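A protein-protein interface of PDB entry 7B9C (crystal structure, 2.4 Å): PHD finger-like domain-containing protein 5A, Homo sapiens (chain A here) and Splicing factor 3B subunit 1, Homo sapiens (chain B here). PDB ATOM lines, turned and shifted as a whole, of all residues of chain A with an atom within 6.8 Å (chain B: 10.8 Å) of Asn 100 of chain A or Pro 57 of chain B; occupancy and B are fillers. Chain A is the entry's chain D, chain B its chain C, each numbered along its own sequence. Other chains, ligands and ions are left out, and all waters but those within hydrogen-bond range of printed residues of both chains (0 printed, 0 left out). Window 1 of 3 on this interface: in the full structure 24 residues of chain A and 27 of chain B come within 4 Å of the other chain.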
ATOM      1  N   ASP A  17       4.381   3.794 -25.433  1.00  0.00           N
ATOM      2  CA  ASP A  17       4.596   3.177 -26.735  1.00  0.00           C
ATOM      3  C   ASP A  17       5.321   1.841 -26.597  1.00  0.00           C
ATOM      4  O   ASP A  17       6.264   1.713 -25.814  1.00  0.00           O
ATOM      5  CB  ASP A  17       5.390   4.113 -27.649  1.00  0.00           C
ATOM      6  CG  ASP A  17       4.965   4.008 -29.102  1.00  0.00           C
ATOM      7  OD1 ASP A  17       3.767   4.221 -29.386  1.00  0.00           O
ATOM      8  OD2 ASP A  17       5.829   3.716 -29.959  1.00  0.00           O
ATOM      9  N   LEU A  18       4.874   0.849 -27.361  1.00  0.00           N
ATOM     10  CA  LEU A  18       5.474  -0.477 -27.363  1.00  0.00           C
ATOM     11  C   LEU A  18       6.473  -0.591 -28.506  1.00  0.00           C
ATOM     12  O   LEU A  18       6.238  -0.068 -29.599  1.00  0.00           O
ATOM     13  CB  LEU A  18       4.402  -1.560 -27.503  1.00  0.00           C
ATOM     14  CG  LEU A  18       3.183  -1.451 -26.589  1.00  0.00           C
ATOM     15  CD1 LEU A  18       2.139  -2.490 -26.975  1.00  0.00           C
ATOM     16  CD2 LEU A  18       3.588  -1.602 -25.130  1.00  0.00           C
ATOM     17  N   ILE A  19       7.589  -1.273 -28.253  1.00  0.00           N
ATOM     18  CA  ILE A  19       8.599  -1.532 -29.273  1.00  0.00           C
ATOM     19  C   ILE A  19       9.111  -2.956 -29.102  1.00  0.00           C
ATOM     20  O   ILE A  19       8.713  -3.678 -28.186  1.00  0.00           O
ATOM     21  CB  ILE A  19       9.777  -0.537 -29.217  1.00  0.00           C
ATOM     22  CG1 ILE A  19      10.424  -0.560 -27.833  1.00  0.00           C
ATOM     23  CG2 ILE A  19       9.332   0.860 -29.621  1.00  0.00           C
ATOM     24  CD1 ILE A  19      11.931  -0.465 -27.876  1.00  0.00           C
ATOM     25  N   ILE A  98       8.237  -7.851 -26.496  1.00  0.00           N
ATOM     26  CA  ILE A  98       7.698  -6.498 -26.597  1.00  0.00           C
ATOM     27  C   ILE A  98       8.000  -5.733 -25.316  1.00  0.00           C
ATOM     28  O   ILE A  98       7.672  -6.183 -24.212  1.00  0.00           O
ATOM     29  CB  ILE A  98       6.189  -6.530 -26.887  1.00  0.00           C
ATOM     30  CG1 ILE A  98       5.950  -6.960 -28.340  1.00  0.00           C
ATOM     31  CG2 ILE A  98       5.554  -5.169 -26.585  1.00  0.00           C
ATOM     32  CD1 ILE A  98       4.598  -6.564 -28.910  1.00  0.00           C
ATOM     33  N   VAL A  99       8.627  -4.570 -25.467  1.00  0.00           N
ATOM     34  CA  VAL A  99       8.979  -3.701 -24.352  1.00  0.00           C
ATOM     35  C   VAL A  99       8.015  -2.524 -24.331  1.00  0.00           C
ATOM     36  O   VAL A  99       7.757  -1.899 -25.372  1.00  0.00           O
ATOM     37  CB  VAL A  99      10.436  -3.216 -24.466  1.00  0.00           C
ATOM     38  CG1 VAL A  99      10.759  -2.229 -23.345  1.00  0.00           C
ATOM     39  CG2 VAL A  99      11.392  -4.396 -24.445  1.00  0.00           C
ATOM     40  N   ASN A 100       7.478  -2.226 -23.148  1.00  0.00           N
ATOM     41  CA  ASN A 100       6.636  -1.056 -22.929  1.00  0.00           C
ATOM     42  C   ASN A 100       7.519   0.077 -22.414  1.00  0.00           C
ATOM     43  O   ASN A 100       7.966   0.049 -21.262  1.00  0.00           O
ATOM     44  CB  ASN A 100       5.517  -1.379 -21.941  1.00  0.00           C
ATOM     45  CG  ASN A 100       4.453  -0.292 -21.872  1.00  0.00           C
ATOM     46  OD1 ASN A 100       4.708   0.873 -22.179  1.00  0.00           O
ATOM     47  ND2 ASN A 100       3.252  -0.675 -21.461  1.00  0.00           N
ATOM     48  N   LEU A 101       7.771   1.074 -23.264  1.00  0.00           N
ATOM     49  CA  LEU A 101       8.659   2.169 -22.890  1.00  0.00           C
ATOM     50  C   LEU A 101       8.022   3.152 -21.913  1.00  0.00           C
ATOM     51  O   LEU A 101       8.726   4.025 -21.397  1.00  0.00           O
ATOM     52  CB  LEU A 101       9.129   2.912 -24.141  1.00  0.00           C
ATOM     53  CG  LEU A 101      10.041   2.109 -25.073  1.00  0.00           C
ATOM     54  CD1 LEU A 101      10.475   2.951 -26.261  1.00  0.00           C
ATOM     55  CD2 LEU A 101      11.249   1.576 -24.317  1.00  0.00           C
ATOM     56  N   GLY A 102       6.723   3.035 -21.645  1.00  0.00           N
ATOM     57  CA  GLY A 102       6.049   3.884 -20.689  1.00  0.00           C
ATOM     58  C   GLY A 102       5.841   3.284 -19.316  1.00  0.00           C
ATOM     59  O   GLY A 102       5.310   3.964 -18.433  1.00  0.00           O
ATOM     60  N   SER A 103       6.246   2.036 -19.103  1.00  0.00           N
ATOM     61  CA  SER A 103       6.046   1.342 -17.840  1.00  0.00           C
ATOM     62  C   SER A 103       7.352   1.256 -17.055  1.00  0.00           C
ATOM     63  O   SER A 103       8.437   1.547 -17.560  1.00  0.00           O
ATOM     64  CB  SER A 103       5.488  -0.065 -18.084  1.00  0.00           C
ATOM     65  OG  SER A 103       4.102  -0.026 -18.375  1.00  0.00           O
ATOM     66  N   SER A 104       7.228   0.848 -15.797  1.00  0.00           N
ATOM     67  CA  SER A 104       8.364   0.508 -14.955  1.00  0.00           C
ATOM     68  C   SER A 104       8.332  -0.990 -14.664  1.00  0.00           C
ATOM     69  O   SER A 104       7.405  -1.703 -15.059  1.00  0.00           O
ATOM     70  CB  SER A 104       8.362   1.347 -13.674  1.00  0.00           C
ATOM     71  OG  SER A 104       7.670   0.697 -12.624  1.00  0.00           O
ATOM     72  N   LYS A 105       9.361  -1.468 -13.958  1.00  0.00           N
ATOM     73  CA  LYS A 105       9.570  -2.909 -13.833  1.00  0.00           C
ATOM     74  C   LYS A 105       8.435  -3.600 -13.083  1.00  0.00           C
ATOM     75  O   LYS A 105       8.170  -4.785 -13.318  1.00  0.00           O
ATOM     76  CB  LYS A 105      10.910  -3.186 -13.147  1.00  0.00           C
ATOM     77  CG  LYS A 105      11.643  -4.409 -13.685  1.00  0.00           C
ATOM     78  CD  LYS A 105      12.498  -4.065 -14.898  1.00  0.00           C
ATOM     79  CE  LYS A 105      13.239  -5.289 -15.409  1.00  0.00           C
ATOM     80  NZ  LYS A 105      14.078  -5.005 -16.606  1.00  0.00           N
ATOM     81  N   LEU A 108       1.624  -2.654 -13.910  1.00  0.00           N
ATOM     82  CA  LEU A 108       0.582  -3.561 -14.396  1.00  0.00           C
ATOM     83  C   LEU A 108       0.518  -4.842 -13.567  1.00  0.00           C
ATOM     84  O   LEU A 108      -0.295  -4.959 -12.649  1.00  0.00           O
ATOM     85  CB  LEU A 108       0.802  -3.901 -15.874  1.00  0.00           C
ATOM     86  CG  LEU A 108       1.069  -2.734 -16.831  1.00  0.00           C
ATOM     87  CD1 LEU A 108       2.526  -2.726 -17.279  1.00  0.00           C
ATOM     88  CD2 LEU A 108       0.136  -2.789 -18.036  1.00  0.00           C
ATOM     89  N   PRO B  13       9.814   9.929 -10.581  1.00  0.00           N
ATOM     90  CA  PRO B  13       8.958   8.744 -10.703  1.00  0.00           C
ATOM     91  C   PRO B  13       8.093   8.538  -9.467  1.00  0.00           C
ATOM     92  O   PRO B  13       8.391   9.018  -8.370  1.00  0.00           O
ATOM     93  CB  PRO B  13       9.957   7.594 -10.879  1.00  0.00           C
ATOM     94  CG  PRO B  13      11.239   8.110 -10.322  1.00  0.00           C
ATOM     95  CD  PRO B  13      11.246   9.586 -10.574  1.00  0.00           C
ATOM     96  N   LEU B  48      19.500   9.123  -8.705  1.00  0.00           N
ATOM     97  CA  LEU B  48      19.871   8.101  -9.680  1.00  0.00           C
ATOM     98  C   LEU B  48      19.272   6.746  -9.316  1.00  0.00           C
ATOM     99  O   LEU B  48      18.727   6.046 -10.179  1.00  0.00           O
ATOM    100  CB  LEU B  48      21.393   8.012  -9.792  1.00  0.00           C
ATOM    101  CG  LEU B  48      22.081   9.174 -10.516  1.00  0.00           C
ATOM    102  CD1 LEU B  48      23.588   9.128 -10.315  1.00  0.00           C
ATOM    103  CD2 LEU B  48      21.738   9.164 -11.996  1.00  0.00           C
ATOM    104  N   LEU B  50      16.606   6.171  -7.514  1.00  0.00           N
ATOM    105  CA  LEU B  50      15.162   6.214  -7.713  1.00  0.00           C
ATOM    106  C   LEU B  50      14.806   6.080  -9.188  1.00  0.00           C
ATOM    107  O   LEU B  50      13.881   5.337  -9.543  1.00  0.00           O
ATOM    108  CB  LEU B  50      14.590   7.508  -7.136  1.00  0.00           C
ATOM    109  CG  LEU B  50      13.083   7.708  -7.300  1.00  0.00           C
ATOM    110  CD1 LEU B  50      12.311   6.529  -6.720  1.00  0.00           C
ATOM    111  CD2 LEU B  50      12.650   9.018  -6.655  1.00  0.00           C
ATOM    112  N   LYS B  51      15.526   6.788 -10.062  1.00  0.00           N
ATOM    113  CA  LYS B  51      15.255   6.676 -11.491  1.00  0.00           C
ATOM    114  C   LYS B  51      15.557   5.276 -12.011  1.00  0.00           C
ATOM    115  O   LYS B  51      14.929   4.826 -12.977  1.00  0.00           O
ATOM    116  CB  LYS B  51      16.060   7.719 -12.268  1.00  0.00           C
ATOM    117  CG  LYS B  51      15.526   9.139 -12.139  1.00  0.00           C
ATOM    118  CD  LYS B  51      16.154  10.067 -13.169  1.00  0.00           C
ATOM    119  CE  LYS B  51      15.532  11.455 -13.113  1.00  0.00           C
ATOM    120  NZ  LYS B  51      16.056  12.344 -14.188  1.00  0.00           N
ATOM    121  N   ILE B  52      16.508   4.574 -11.390  1.00  0.00           N
ATOM    122  CA  ILE B  52      16.812   3.212 -11.822  1.00  0.00           C
ATOM    123  C   ILE B  52      15.733   2.244 -11.348  1.00  0.00           C
ATOM    124  O   ILE B  52      15.272   1.386 -12.110  1.00  0.00           O
ATOM    125  CB  ILE B  52      18.208   2.789 -11.328  1.00  0.00           C
ATOM    126  CG1 ILE B  52      19.300   3.532 -12.098  1.00  0.00           C
ATOM    127  CG2 ILE B  52      18.401   1.286 -11.478  1.00  0.00           C
ATOM    128  CD1 ILE B  52      20.689   3.338 -11.527  1.00  0.00           C
ATOM    129  N   LYS B  53      15.300   2.372 -10.091  1.00  0.00           N
ATOM    130  CA  LYS B  53      14.368   1.396  -9.535  1.00  0.00           C
ATOM    131  C   LYS B  53      12.944   1.602 -10.039  1.00  0.00           C
ATOM    132  O   LYS B  53      12.238   0.627 -10.318  1.00  0.00           O
ATOM    133  CB  LYS B  53      14.395   1.444  -8.007  1.00  0.00           C
ATOM    134  CG  LYS B  53      13.638   0.297  -7.353  1.00  0.00           C
ATOM    135  CD  LYS B  53      13.785   0.313  -5.839  1.00  0.00           C
ATOM    136  CE  LYS B  53      12.755   1.222  -5.199  1.00  0.00           C
ATOM    137  NZ  LYS B  53      11.373   0.754  -5.490  1.00  0.00           N
ATOM    138  N   ASN B  54      12.497   2.852 -10.153  1.00  0.00           N
ATOM    139  CA  ASN B  54      11.104   3.149 -10.451  1.00  0.00           C
ATOM    140  C   ASN B  54      10.895   3.768 -11.827  1.00  0.00           C
ATOM    141  O   ASN B  54       9.747   4.017 -12.210  1.00  0.00           O
ATOM    142  CB  ASN B  54      10.526   4.082  -9.378  1.00  0.00           C
ATOM    143  CG  ASN B  54      10.429   3.419  -8.015  1.00  0.00           C
ATOM    144  OD1 ASN B  54      11.050   2.384  -7.767  1.00  0.00           O
ATOM    145  ND2 ASN B  54       9.643   4.014  -7.124  1.00  0.00           N
ATOM    146  N   GLY B  55      11.963   4.018 -12.583  1.00  0.00           N
ATOM    147  CA  GLY B  55      11.830   4.723 -13.838  1.00  0.00           C
ATOM    148  C   GLY B  55      11.447   3.829 -15.005  1.00  0.00           C
ATOM    149  O   GLY B  55      11.432   2.601 -14.917  1.00  0.00           O
ATOM    150  N   THR B  56      11.125   4.486 -16.120  1.00  0.00           N
ATOM    151  CA  THR B  56      10.862   3.812 -17.379  1.00  0.00           C
ATOM    152  C   THR B  56      12.176   3.283 -17.953  1.00  0.00           C
ATOM    153  O   THR B  56      13.255   3.653 -17.486  1.00  0.00           O
ATOM    154  CB  THR B  56      10.178   4.775 -18.351  1.00  0.00           C
ATOM    155  OG1 THR B  56      11.013   5.918 -18.566  1.00  0.00           O
ATOM    156  CG2 THR B  56       8.840   5.228 -17.791  1.00  0.00           C
ATOM    157  N   PRO B  57      12.120   2.396 -18.948  1.00  0.00           N
ATOM    158  CA  PRO B  57      13.358   1.847 -19.532  1.00  0.00           C
ATOM    159  C   PRO B  57      14.329   2.930 -19.980  1.00  0.00           C
ATOM    160  O   PRO B  57      15.536   2.809 -19.718  1.00  0.00           O
ATOM    161  CB  PRO B  57      12.850   1.010 -20.714  1.00  0.00           C
ATOM    162  CG  PRO B  57      11.510   0.550 -20.267  1.00  0.00           C
ATOM    163  CD  PRO B  57      10.930   1.668 -19.433  1.00  0.00           C
ATOM    164  N   PRO B  58      13.877   4.005 -20.648  1.00  0.00           N
ATOM    165  CA  PRO B  58      14.845   5.066 -20.983  1.00  0.00           C
ATOM    166  C   PRO B  58      15.430   5.748 -19.758  1.00  0.00           C
ATOM    167  O   PRO B  58      16.638   6.033 -19.723  1.00  0.00           O
ATOM    168  CB  PRO B  58      14.022   6.038 -21.844  1.00  0.00           C
ATOM    169  CG  PRO B  58      12.613   5.768 -21.480  1.00  0.00           C
ATOM    170  CD  PRO B  58      12.556   4.297 -21.240  1.00  0.00           C
ATOM    171  N   MET B  59      14.602   6.018 -18.747  1.00  0.00           N
ATOM    172  CA  MET B  59      15.108   6.601 -17.509  1.00  0.00           C
ATOM    173  C   MET B  59      16.106   5.670 -16.833  1.00  0.00           C
ATOM    174  O   MET B  59      17.160   6.117 -16.362  1.00  0.00           O
ATOM    175  CB  MET B  59      13.949   6.918 -16.563  1.00  0.00           C
ATOM    176  CG  MET B  59      12.975   7.961 -17.083  1.00  0.00           C
ATOM    177  SD  MET B  59      11.551   8.148 -15.987  1.00  0.00           S
ATOM    178  CE  MET B  59      12.365   8.588 -14.450  1.00  0.00           C
ATOM    179  N   ARG B  60      15.786   4.375 -16.764  1.00  0.00           N
ATOM    180  CA  ARG B  60      16.717   3.415 -16.178  1.00  0.00           C
ATOM    181  C   ARG B  60      18.037   3.402 -16.935  1.00  0.00           C
ATOM    182  O   ARG B  60      19.110   3.405 -16.323  1.00  0.00           O
ATOM    183  CB  ARG B  60      16.100   2.014 -16.161  1.00  0.00           C
ATOM    184  CG  ARG B  60      14.834   1.885 -15.330  1.00  0.00           C
ATOM    185  CD  ARG B  60      14.539   0.429 -14.990  1.00  0.00           C
ATOM    186  NE  ARG B  60      14.509  -0.430 -16.172  1.00  0.00           N
ATOM    187  CZ  ARG B  60      13.398  -0.882 -16.744  1.00  0.00           C
ATOM    188  NH1 ARG B  60      12.210  -0.558 -16.247  1.00  0.00           N
ATOM    189  NH2 ARG B  60      13.471  -1.660 -17.817  1.00  0.00           N
ATOM    190  N   LYS B  61      17.977   3.397 -18.270  1.00  0.00           N
ATOM    191  CA  LYS B  61      19.195   3.368 -19.076  1.00  0.00           C
ATOM    192  C   LYS B  61      20.052   4.600 -18.816  1.00  0.00           C
ATOM    193  O   LYS B  61      21.260   4.491 -18.564  1.00  0.00           O
ATOM    194  CB  LYS B  61      18.830   3.262 -20.557  1.00  0.00           C
ATOM    195  CG  LYS B  61      19.996   2.947 -21.480  1.00  0.00           C
ATOM    196  CD  LYS B  61      19.514   2.682 -22.900  1.00  0.00           C
ATOM    197  CE  LYS B  61      20.617   2.081 -23.762  1.00  0.00           C
ATOM    198  NZ  LYS B  61      20.098   1.596 -25.074  1.00  0.00           N
ATOM    199  N   ALA B  62      19.438   5.785 -18.863  1.00  0.00           N
ATOM    200  CA  ALA B  62      20.188   7.020 -18.652  1.00  0.00           C
ATOM    201  C   ALA B  62      20.791   7.068 -17.253  1.00  0.00           C
ATOM    202  O   ALA B  62      21.973   7.399 -17.084  1.00  0.00           O
ATOM    203  CB  ALA B  62      19.282   8.228 -18.893  1.00  0.00           C
ATOM    204  N   ALA B  63      19.996   6.734 -16.232  1.00  0.00           N
ATOM    205  CA  ALA B  63      20.485   6.811 -14.859  1.00  0.00           C
ATOM    206  C   ALA B  63      21.582   5.787 -14.602  1.00  0.00           C
ATOM    207  O   ALA B  63      22.553   6.077 -13.893  1.00  0.00           O
ATOM    208  CB  ALA B  63      19.330   6.625 -13.878  1.00  0.00           C
ATOM    209  N   LEU B  64      21.455   4.588 -15.175  1.00  0.00           N
ATOM    210  CA  LEU B  64      22.504   3.585 -15.041  1.00  0.00           C
ATOM    211  C   LEU B  64      23.793   4.060 -15.693  1.00  0.00           C
ATOM    212  O   LEU B  64      24.877   3.957 -15.104  1.00  0.00           O
ATOM    213  CB  LEU B  64      22.038   2.263 -15.652  1.00  0.00           C
ATOM    214  CG  LEU B  64      23.082   1.154 -15.800  1.00  0.00           C
ATOM    215  CD1 LEU B  64      23.531   0.658 -14.434  1.00  0.00           C
ATOM    216  CD2 LEU B  64      22.540   0.006 -16.642  1.00  0.00           C
ATOM    217  N   ARG B  65      23.695   4.600 -16.911  1.00  0.00           N
ATOM    218  CA  ARG B  65      24.888   5.095 -17.588  1.00  0.00           C
ATOM    219  C   ARG B  65      25.557   6.201 -16.782  1.00  0.00           C
ATOM    220  O   ARG B  65      26.787   6.228 -16.654  1.00  0.00           O
ATOM    221  CB  ARG B  65      24.532   5.588 -18.992  1.00  0.00           C
ATOM    222  CG  ARG B  65      25.732   5.994 -19.837  1.00  0.00           C
ATOM    223  CD  ARG B  65      25.813   7.504 -19.986  1.00  0.00           C
ATOM    224  NE  ARG B  65      26.370   7.907 -21.274  1.00  0.00           N
ATOM    225  CZ  ARG B  65      25.654   8.061 -22.384  1.00  0.00           C
ATOM    226  NH1 ARG B  65      24.346   7.842 -22.370  1.00  0.00           N
ATOM    227  NH2 ARG B  65      26.247   8.435 -23.511  1.00  0.00           N
ATOM    228  N   GLN B  66      24.763   7.106 -16.206  1.00  0.00           N
ATOM    229  CA  GLN B  66      25.355   8.231 -15.490  1.00  0.00           C
ATOM    230  C   GLN B  66      25.927   7.811 -14.138  1.00  0.00           C
ATOM    231  O   GLN B  66      26.953   8.349 -13.709  1.00  0.00           O
ATOM    232  CB  GLN B  66      24.330   9.351 -15.321  1.00  0.00           C
ATOM    233  CG  GLN B  66      24.611  10.564 -16.206  1.00  0.00           C
ATOM    234  CD  GLN B  66      25.008  10.182 -17.629  1.00  0.00           C
ATOM    235  OE1 GLN B  66      24.160   9.818 -18.446  1.00  0.00           O
ATOM    236  NE2 GLN B  66      26.300  10.269 -17.929  1.00  0.00           N
ATOM    237  N   LEU B  99      17.833  -5.459 -10.866  1.00  0.00           N
ATOM    238  CA  LEU B  99      18.306  -4.144 -11.290  1.00  0.00           C
ATOM    239  C   LEU B  99      19.419  -3.646 -10.380  1.00  0.00           C
ATOM    240  O   LEU B  99      20.452  -3.150 -10.848  1.00  0.00           O
ATOM    241  CB  LEU B  99      17.146  -3.150 -11.296  1.00  0.00           C
ATOM    242  CG  LEU B  99      16.244  -3.127 -12.526  1.00  0.00           C
ATOM    243  CD1 LEU B  99      15.178  -2.055 -12.364  1.00  0.00           C
ATOM    244  CD2 LEU B  99      17.068  -2.889 -13.776  1.00  0.00           C
ATOM    245  N   LYS B 102      22.627  -5.525 -11.017  1.00  0.00           N
ATOM    246  CA  LYS B 102      23.299  -5.019 -12.212  1.00  0.00           C
ATOM    247  C   LYS B 102      23.997  -3.694 -11.930  1.00  0.00           C
ATOM    248  O   LYS B 102      25.110  -3.447 -12.418  1.00  0.00           O
ATOM    249  CB  LYS B 102      22.290  -4.866 -13.350  1.00  0.00           C
ATOM    250  CG  LYS B 102      22.902  -4.445 -14.675  1.00  0.00           C
ATOM    251  CD  LYS B 102      21.836  -3.999 -15.667  1.00  0.00           C
ATOM    252  CE  LYS B 102      22.118  -4.558 -17.055  1.00  0.00           C
ATOM    253  NZ  LYS B 102      20.956  -4.488 -17.987  1.00  0.00           N
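SD of Met 59 of chain B lies close to OG1 of Thr 56 of chain B (3.5 Å).
OD1 of Asn 100 of chain A sits at hydrogen-bond distance from N of Gly 102 of chain A (3.0 Å).
The side-chain amide oxygen (OD1) of Asn 54 of chain B is in hydrogen-bond range of the side-chain amino group (NZ) of Lys 53 of chain B, 2.8 Å away.
The side-chain amide nitrogen of Asn 100 of chain A sits at hydrogen-bond distance from the side-chain hydroxyl of Ser 103 of chain A (3.3 Å).
O of Asp 17 of chain A is in hydrogen-bond range of N of Leu 101 of chain A (3.0 Å).
Asn 100 of chain A touches Pro 57 of chain B (O to CG, 3.7 Å).
Thr 56 of chain B touches Leu 101 of chain A.
O of Leu 101 of chain A touches CD of Pro 57 of chain B, at 3.8 Å.
CD of Pro 58 of chain B touches O of Leu 101 of chain A, at 3.8 Å.
Gly 102 of chain A touches Thr 56 of chain B (O to CG2, 3.8 Å).
Thr 56 of chain B touches Ser 103 of chain A.
Pro 57 of chain B touches Ser 103 of chain A.
O of Asn 54 of chain B touches CB of Ser 104 of chain A, 3.3 Å away.
Ser 104 of chain A touches Gly 55 of chain B.
Lys 105 of chain A touches Arg 60 of chain B (NZ to NH2, 3.6 Å).
Ile 98 of chain A touches none of the printed residues of chain B.
No residue of chain B comes within 4 Å of Val 99 of chain A.
Asn 100 of chain A touches just one residue of chain B: Pro 57.
Leu 101 of chain A touches just these residues of chain B: Thr 56 (3.5 Å), Pro 57 (3.8 Å) and Pro 58 (3.8 Å).
Of chain B, only Thr 56 (3.8 Å) comes within 4 Å of Gly 102 of chain A.
Of chain B, only Thr 56 (3.3 Å) and Pro 57 (3.1 Å) come within 4 Å of Ser 103 of chain A.
Of the printed residues of chain B, Ser 104 of chain A touches Asn 54 (3.3 Å) and Gly 55 (3.5 Å).
Of the printed residues of chain B, Lys 105 of chain A touches Arg 60.
Of the printed residues of chain A, Thr 56 of chain B touches Leu 101, Gly 102 and Ser 103.
Pro 57 of chain B touches just these residues of chain A: Asn 100, Leu 101 and Ser 103.
Met 59 of chain B touches none of the printed residues of chain A.
The nearest residue of chain B that does not touch Asn 100 of chain A is Thr 56 of chain B (6.0 Å).
The nearest printed residue of chain A that does not touch Pro 58 of chain B is Gly 102 of chain A (6.0 Å).
Of the 12 printed residues of chain A, 6 touch a printed residue of chain B.
Hydrophobic or aromatic side chains of chain A that line the printed part of chain B: Leu 101.
Of the 21 printed residues of chain B, 6 touch a printed residue of chain A.
Printed residues of chain B that touch a printed residue of chain A: Asn 54, Gly 55, Thr 56, Pro 57, Pro 58 and Arg 60.
Along chain B the printed residues that touch a printed residue of chain A span positions 54 to 60.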
